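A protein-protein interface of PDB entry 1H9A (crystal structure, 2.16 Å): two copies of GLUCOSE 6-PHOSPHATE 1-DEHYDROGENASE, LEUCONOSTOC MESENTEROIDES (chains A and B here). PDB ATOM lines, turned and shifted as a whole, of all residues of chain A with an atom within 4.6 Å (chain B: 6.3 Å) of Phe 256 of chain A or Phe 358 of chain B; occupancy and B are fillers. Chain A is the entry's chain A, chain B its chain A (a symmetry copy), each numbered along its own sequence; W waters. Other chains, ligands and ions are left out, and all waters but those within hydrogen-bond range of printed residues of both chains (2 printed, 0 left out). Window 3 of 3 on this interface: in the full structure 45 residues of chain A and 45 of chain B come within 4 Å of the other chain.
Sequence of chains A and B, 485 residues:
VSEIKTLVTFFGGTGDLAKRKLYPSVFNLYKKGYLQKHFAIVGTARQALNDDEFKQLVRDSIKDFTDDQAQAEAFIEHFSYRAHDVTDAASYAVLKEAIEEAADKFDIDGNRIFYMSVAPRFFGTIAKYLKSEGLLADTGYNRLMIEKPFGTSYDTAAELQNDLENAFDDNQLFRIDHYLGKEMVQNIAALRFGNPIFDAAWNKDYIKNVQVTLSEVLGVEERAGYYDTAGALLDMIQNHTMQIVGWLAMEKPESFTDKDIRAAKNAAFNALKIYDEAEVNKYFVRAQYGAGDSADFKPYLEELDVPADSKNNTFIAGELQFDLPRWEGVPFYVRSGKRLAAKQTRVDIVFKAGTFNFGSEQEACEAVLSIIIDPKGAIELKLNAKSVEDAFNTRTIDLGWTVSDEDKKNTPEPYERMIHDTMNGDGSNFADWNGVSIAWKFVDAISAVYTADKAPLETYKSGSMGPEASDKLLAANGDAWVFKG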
ATOM      1  N   ALA A 189       0.625 -18.575 -17.036  1.00  0.00           N
ATOM      2  CA  ALA A 189       1.761 -19.217 -16.387  1.00  0.00           C
ATOM      3  C   ALA A 189       1.660 -20.744 -16.432  1.00  0.00           C
ATOM      4  O   ALA A 189       2.677 -21.433 -16.559  1.00  0.00           O
ATOM      5  CB  ALA A 189       1.903 -18.724 -14.953  1.00  0.00           C
ATOM      6  N   ALA A 190       0.441 -21.271 -16.362  1.00  0.00           N
ATOM      7  CA  ALA A 190       0.232 -22.718 -16.419  1.00  0.00           C
ATOM      8  C   ALA A 190       0.589 -23.262 -17.806  1.00  0.00           C
ATOM      9  O   ALA A 190       1.294 -24.266 -17.924  1.00  0.00           O
ATOM     10  CB  ALA A 190      -1.199 -23.060 -16.070  1.00  0.00           C
ATOM     11  N   PHE A 193       4.839 -22.518 -18.329  1.00  0.00           N
ATOM     12  CA  PHE A 193       5.704 -23.360 -17.504  1.00  0.00           C
ATOM     13  C   PHE A 193       5.312 -24.812 -17.329  1.00  0.00           C
ATOM     14  O   PHE A 193       6.157 -25.632 -16.980  1.00  0.00           O
ATOM     15  CB  PHE A 193       5.896 -22.721 -16.133  1.00  0.00           C
ATOM     16  CG  PHE A 193       6.428 -21.326 -16.194  1.00  0.00           C
ATOM     17  CD1 PHE A 193       7.613 -21.050 -16.875  1.00  0.00           C
ATOM     18  CD2 PHE A 193       5.733 -20.276 -15.601  1.00  0.00           C
ATOM     19  CE1 PHE A 193       8.099 -19.747 -16.966  1.00  0.00           C
ATOM     20  CE2 PHE A 193       6.208 -18.972 -15.687  1.00  0.00           C
ATOM     21  CZ  PHE A 193       7.393 -18.705 -16.372  1.00  0.00           C
ATOM     22  N   GLY A 194       4.037 -25.120 -17.556  1.00  0.00           N
ATOM     23  CA  GLY A 194       3.554 -26.480 -17.398  1.00  0.00           C
ATOM     24  C   GLY A 194       3.746 -27.376 -18.608  1.00  0.00           C
ATOM     25  O   GLY A 194       3.513 -28.579 -18.528  1.00  0.00           O
ATOM     26  N   TRP A 247       2.922 -10.697 -16.925  1.00  0.00           N
ATOM     27  CA  TRP A 247       2.820 -12.151 -16.912  1.00  0.00           C
ATOM     28  C   TRP A 247       3.484 -12.761 -18.145  1.00  0.00           C
ATOM     29  O   TRP A 247       4.138 -13.797 -18.057  1.00  0.00           O
ATOM     30  CB  TRP A 247       1.354 -12.595 -16.869  1.00  0.00           C
ATOM     31  CG  TRP A 247       0.804 -12.743 -15.491  1.00  0.00           C
ATOM     32  CD1 TRP A 247      -0.216 -12.029 -14.935  1.00  0.00           C
ATOM     33  CD2 TRP A 247       1.237 -13.675 -14.487  1.00  0.00           C
ATOM     34  NE1 TRP A 247      -0.445 -12.456 -13.649  1.00  0.00           N
ATOM     35  CE2 TRP A 247       0.430 -13.466 -13.349  1.00  0.00           C
ATOM     36  CE3 TRP A 247       2.230 -14.667 -14.442  1.00  0.00           C
ATOM     37  CZ2 TRP A 247       0.582 -14.213 -12.173  1.00  0.00           C
ATOM     38  CZ3 TRP A 247       2.382 -15.411 -13.271  1.00  0.00           C
ATOM     39  CH2 TRP A 247       1.559 -15.178 -12.152  1.00  0.00           C
ATOM     40  N   SER A 255      10.819 -20.630  -8.418  1.00  0.00           N
ATOM     41  CA  SER A 255       9.748 -21.455  -7.873  1.00  0.00           C
ATOM     42  C   SER A 255       8.472 -20.664  -8.115  1.00  0.00           C
ATOM     43  O   SER A 255       8.540 -19.508  -8.537  1.00  0.00           O
ATOM     44  CB  SER A 255       9.954 -21.728  -6.375  1.00  0.00           C
ATOM     45  OG  SER A 255       9.603 -20.615  -5.570  1.00  0.00           O
ATOM     46  N   PHE A 256       7.319 -21.277  -7.888  1.00  0.00           N
ATOM     47  CA  PHE A 256       6.064 -20.582  -8.101  1.00  0.00           C
ATOM     48  C   PHE A 256       5.526 -19.864  -6.858  1.00  0.00           C
ATOM     49  O   PHE A 256       4.316 -19.819  -6.626  1.00  0.00           O
ATOM     50  CB  PHE A 256       5.017 -21.532  -8.682  1.00  0.00           C
ATOM     51  CG  PHE A 256       4.029 -20.849  -9.573  1.00  0.00           C
ATOM     52  CD1 PHE A 256       4.462 -20.144 -10.691  1.00  0.00           C
ATOM     53  CD2 PHE A 256       2.671 -20.874  -9.283  1.00  0.00           C
ATOM     54  CE1 PHE A 256       3.555 -19.469 -11.509  1.00  0.00           C
ATOM     55  CE2 PHE A 256       1.758 -20.203 -10.093  1.00  0.00           C
ATOM     56  CZ  PHE A 256       2.203 -19.497 -11.209  1.00  0.00           C
ATOM     57  N   THR A 257       6.428 -19.311  -6.053  1.00  0.00           N
ATOM     58  CA  THR A 257       6.027 -18.575  -4.855  1.00  0.00           C
ATOM     59  C   THR A 257       5.829 -17.113  -5.269  1.00  0.00           C
ATOM     60  O   THR A 257       6.525 -16.628  -6.165  1.00  0.00           O
ATOM     61  CB  THR A 257       7.113 -18.649  -3.741  1.00  0.00           C
ATOM     62  OG1 THR A 257       8.346 -18.087  -4.213  1.00  0.00           O
ATOM     63  CG2 THR A 257       7.346 -20.092  -3.310  1.00  0.00           C
ATOM     64  N   ASP A 258       4.912 -16.405  -4.614  1.00  0.00           N
ATOM     65  CA  ASP A 258       4.660 -15.002  -4.950  1.00  0.00           C
ATOM     66  C   ASP A 258       5.928 -14.136  -5.013  1.00  0.00           C
ATOM     67  O   ASP A 258       6.069 -13.297  -5.907  1.00  0.00           O
ATOM     68  CB  ASP A 258       3.611 -14.380  -4.006  1.00  0.00           C
ATOM     69  CG  ASP A 258       3.964 -14.519  -2.519  1.00  0.00           C
ATOM     70  OD1 ASP A 258       5.044 -15.056  -2.181  1.00  0.00           O
ATOM     71  OD2 ASP A 258       3.143 -14.080  -1.679  1.00  0.00           O
ATOM     72  N   ILE A 261       7.813 -15.086  -8.220  1.00  0.00           N
ATOM     73  CA  ILE A 261       7.063 -14.641  -9.386  1.00  0.00           C
ATOM     74  C   ILE A 261       7.297 -13.139  -9.570  1.00  0.00           C
ATOM     75  O   ILE A 261       7.569 -12.679 -10.684  1.00  0.00           O
ATOM     76  CB  ILE A 261       5.557 -14.948  -9.241  1.00  0.00           C
ATOM     77  CG1 ILE A 261       5.338 -16.464  -9.301  1.00  0.00           C
ATOM     78  CG2 ILE A 261       4.746 -14.226 -10.321  1.00  0.00           C
ATOM     79  CD1 ILE A 261       3.910 -16.896  -9.054  1.00  0.00           C
ATOM     80  N   PHE B 356       8.867 -28.304 -13.748  1.00  0.00           N
ATOM     81  CA  PHE B 356       8.616 -27.065 -13.034  1.00  0.00           C
ATOM     82  C   PHE B 356       7.675 -27.359 -11.877  1.00  0.00           C
ATOM     83  O   PHE B 356       6.652 -28.020 -12.046  1.00  0.00           O
ATOM     84  CB  PHE B 356       8.008 -26.000 -13.949  1.00  0.00           C
ATOM     85  CG  PHE B 356       7.901 -24.649 -13.304  1.00  0.00           C
ATOM     86  CD1 PHE B 356       9.041 -23.876 -13.089  1.00  0.00           C
ATOM     87  CD2 PHE B 356       6.673 -24.164 -12.871  1.00  0.00           C
ATOM     88  CE1 PHE B 356       8.962 -22.642 -12.448  1.00  0.00           C
ATOM     89  CE2 PHE B 356       6.580 -22.934 -12.229  1.00  0.00           C
ATOM     90  CZ  PHE B 356       7.730 -22.169 -12.015  1.00  0.00           C
ATOM     91  N   ASN B 357       8.025 -26.866 -10.699  1.00  0.00           N
ATOM     92  CA  ASN B 357       7.217 -27.086  -9.514  1.00  0.00           C
ATOM     93  C   ASN B 357       6.254 -25.934  -9.226  1.00  0.00           C
ATOM     94  O   ASN B 357       6.676 -24.809  -8.965  1.00  0.00           O
ATOM     95  CB  ASN B 357       8.132 -27.332  -8.310  1.00  0.00           C
ATOM     96  CG  ASN B 357       7.365 -27.449  -7.004  1.00  0.00           C
ATOM     97  OD1 ASN B 357       7.661 -26.754  -6.029  1.00  0.00           O
ATOM     98  ND2 ASN B 357       6.363 -28.325  -6.979  1.00  0.00           N
ATOM     99  N   PHE B 358       4.956 -26.215  -9.314  1.00  0.00           N
ATOM    100  CA  PHE B 358       3.929 -25.216  -9.026  1.00  0.00           C
ATOM    101  C   PHE B 358       3.609 -25.217  -7.527  1.00  0.00           C
ATOM    102  O   PHE B 358       3.041 -24.259  -7.004  1.00  0.00           O
ATOM    103  CB  PHE B 358       2.640 -25.519  -9.806  1.00  0.00           C
ATOM    104  CG  PHE B 358       2.728 -25.223 -11.280  1.00  0.00           C
ATOM    105  CD1 PHE B 358       2.650 -23.912 -11.746  1.00  0.00           C
ATOM    106  CD2 PHE B 358       2.885 -26.258 -12.207  1.00  0.00           C
ATOM    107  CE1 PHE B 358       2.727 -23.632 -13.109  1.00  0.00           C
ATOM    108  CE2 PHE B 358       2.963 -25.990 -13.576  1.00  0.00           C
ATOM    109  CZ  PHE B 358       2.884 -24.674 -14.027  1.00  0.00           C
ATOM    110  N   GLY B 359       3.998 -26.290  -6.842  1.00  0.00           N
ATOM    111  CA  GLY B 359       3.712 -26.418  -5.425  1.00  0.00           C
ATOM    112  C   GLY B 359       2.258 -26.830  -5.254  1.00  0.00           C
ATOM    113  O   GLY B 359       1.698 -26.754  -4.155  1.00  0.00           O
ATOM    114  N   SER B 360       1.650 -27.266  -6.358  1.00  0.00           N
ATOM    115  CA  SER B 360       0.251 -27.690  -6.391  1.00  0.00           C
ATOM    116  C   SER B 360       0.109 -29.160  -6.020  1.00  0.00           C
ATOM    117  O   SER B 360       1.106 -29.894  -5.981  1.00  0.00           O
ATOM    118  CB  SER B 360      -0.326 -27.459  -7.797  1.00  0.00           C
ATOM    119  OG  SER B 360       0.541 -27.968  -8.806  1.00  0.00           O
ATOM    120  N   GLN B 362      -1.698 -31.410  -7.789  1.00  0.00           N
ATOM    121  CA  GLN B 362      -1.538 -32.094  -9.070  1.00  0.00           C
ATOM    122  C   GLN B 362      -0.492 -31.340  -9.908  1.00  0.00           C
ATOM    123  O   GLN B 362      -0.687 -30.165 -10.271  1.00  0.00           O
ATOM    124  CB  GLN B 362      -2.878 -32.156  -9.818  1.00  0.00           C
ATOM    125  CG  GLN B 362      -2.797 -32.751 -11.228  1.00  0.00           C
ATOM    126  CD  GLN B 362      -2.226 -34.166 -11.248  1.00  0.00           C
ATOM    127  OE1 GLN B 362      -1.007 -34.361 -11.199  1.00  0.00           O
ATOM    128  NE2 GLN B 362      -3.107 -35.159 -11.317  1.00  0.00           N
ATOM    129  N   GLU B 363       0.646 -31.990 -10.136  1.00  0.00           N
ATOM    130  CA  GLU B 363       1.716 -31.399 -10.930  1.00  0.00           C
ATOM    131  C   GLU B 363       1.487 -31.640 -12.420  1.00  0.00           C
ATOM    132  O   GLU B 363       0.574 -32.375 -12.803  1.00  0.00           O
ATOM    133  CB  GLU B 363       3.081 -31.941 -10.500  1.00  0.00           C
ATOM    134  CG  GLU B 363       3.584 -31.349  -9.187  1.00  0.00           C
ATOM    135  CD  GLU B 363       3.746 -29.823  -9.222  1.00  0.00           C
ATOM    136  OE1 GLU B 363       3.847 -29.232 -10.327  1.00  0.00           O
ATOM    137  OE2 GLU B 363       3.783 -29.214  -8.130  1.00  0.00           O
ATOM    138  N   ALA B 364       2.312 -31.009 -13.251  1.00  0.00           N
ATOM    139  CA  ALA B 364       2.195 -31.134 -14.701  1.00  0.00           C
ATOM    140  C   ALA B 364       2.308 -32.571 -15.207  1.00  0.00           C
ATOM    141  O   ALA B 364       3.244 -33.293 -14.866  1.00  0.00           O
ATOM    142  CB  ALA B 364       3.229 -30.244 -15.390  1.00  0.00           C
ATOM    143  N   PHE B 392      -4.356 -22.812  -6.648  1.00  0.00           N
ATOM    144  CA  PHE B 392      -3.732 -23.018  -7.946  1.00  0.00           C
ATOM    145  C   PHE B 392      -3.371 -24.492  -8.100  1.00  0.00           C
ATOM    146  O   PHE B 392      -2.735 -25.086  -7.222  1.00  0.00           O
ATOM    147  CB  PHE B 392      -2.477 -22.154  -8.107  1.00  0.00           C
ATOM    148  CG  PHE B 392      -1.920 -22.158  -9.505  1.00  0.00           C
ATOM    149  CD1 PHE B 392      -1.131 -23.215  -9.954  1.00  0.00           C
ATOM    150  CD2 PHE B 392      -2.219 -21.124 -10.389  1.00  0.00           C
ATOM    151  CE1 PHE B 392      -0.654 -23.244 -11.259  1.00  0.00           C
ATOM    152  CE2 PHE B 392      -1.744 -21.144 -11.700  1.00  0.00           C
ATOM    153  CZ  PHE B 392      -0.961 -22.207 -12.135  1.00  0.00           C
ATOM    154  N   ASN B 393      -3.754 -25.061  -9.236  1.00  0.00           N
ATOM    155  CA  ASN B 393      -3.502 -26.462  -9.524  1.00  0.00           C
ATOM    156  C   ASN B 393      -3.560 -26.629 -11.036  1.00  0.00           C
ATOM    157  O   ASN B 393      -4.099 -25.760 -11.731  1.00  0.00           O
ATOM    158  CB  ASN B 393      -4.589 -27.309  -8.860  1.00  0.00           C
ATOM    159  CG  ASN B 393      -4.227 -28.769  -8.785  1.00  0.00           C
ATOM    160  OD1 ASN B 393      -3.081 -29.116  -8.512  1.00  0.00           O
ATOM    161  ND2 ASN B 393      -5.207 -29.638  -8.995  1.00  0.00           N
ATOM    162  N   THR B 394      -3.004 -27.726 -11.547  1.00  0.00           N
ATOM    163  CA  THR B 394      -2.999 -27.992 -12.985  1.00  0.00           C
ATOM    164  C   THR B 394      -4.007 -29.066 -13.388  1.00  0.00           C
ATOM    165  O   THR B 394      -4.474 -29.845 -12.552  1.00  0.00           O
ATOM    166  CB  THR B 394      -1.586 -28.408 -13.490  1.00  0.00           C
ATOM    167  OG1 THR B 394      -1.180 -29.630 -12.862  1.00  0.00           O
ATOM    168  CG2 THR B 394      -0.569 -27.325 -13.184  1.00  0.00           C
HETATM  169  O   HOH W   1       7.156 -23.545  -6.395  1.00  0.00           O
HETATM  170  O   HOH W   2       6.529 -28.290 -15.906  1.00  0.00           O
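N of Gly 359 of chain B sits close to ND2 of Asn 357 of chain B, 3.1 Å away. The side-chain amide nitrogen (ND2) of Asn 357 of chain B lies within hydrogen-bond range of the side-chain carboxylate (OE2) of Glu 363 of chain B (3.0 Å). OE1 of Glu 363 of chain B lies within hydrogen-bond range of N of Phe 358 of chain B (3.4 Å).
Phe 356 of chain B touches Phe 193 of chain A (CB to O, 3.6 Å). Gly 194 of chain A touches Phe 358 of chain B (N to CZ, 3.7 Å). Gly 194 of chain A touches Ala 364 of chain B (O to CB, 3.6 Å). Phe 256 of chain A touches Phe 356 of chain B (CD1 to CE2, 3.8 Å). Asn 357 of chain B touches Phe 256 of chain A. CB of Phe 256 of chain A touches O of Phe 358 of chain B (3.8 Å). Phe 256 of chain A touches Phe 392 of chain B (CE2 to CZ, 3.9 Å).
Of the printed residues of chain B, Phe 256 of chain A touches Phe 356 (3.8 Å), Asn 357 (3.7 Å), Phe 358 (3.8 Å) and Phe 392 (3.9 Å). Of chain A, only Gly 194 and Phe 256 come within 4 Å of Phe 358 of chain B. Printed residues of chain A within 4 Å of Asn 357 of chain B: Phe 256. Of the printed residues of chain B, Gly 194 of chain A touches Phe 358 (3.7 Å) and Ala 364 (3.6 Å). Of the printed residues of chain A, Phe 392 of chain B touches Phe 256 (3.9 Å). Asn 393 of chain B touches none of the printed residues of chain A. The nearest printed residue of chain A that does not touch Phe 358 of chain B is Ala 190 of chain A (4.1 Å). The nearest printed residue of chain A that does not touch Ala 364 of chain B is Phe 193 of chain A (5.7 Å).
Hydrophobic or aromatic side chains of chain B that line the printed part of chain A: Phe 356, Phe 358, Ala 364 and Phe 392. Printed residues of chain A that touch a printed residue of chain B: Phe 193, Gly 194 and Phe 256. Among the printed residues, no Asp or Glu carboxylate lies within 4 Å of a Lys or Arg side-chain nitrogen of the other chain.
No position is printed for both chains.
Water W1 lies within hydrogen-bond range of the backbone NH (N) of Phe 256 of chain A (2.7 Å) and the backbone carbonyl oxygen (O) of Asn 357 of chain B (2.9 Å). Water W2 lies within hydrogen-bond range of the backbone carbonyl oxygen of Phe 193 of chain A and the backbone NH of Phe 356 of chain B.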
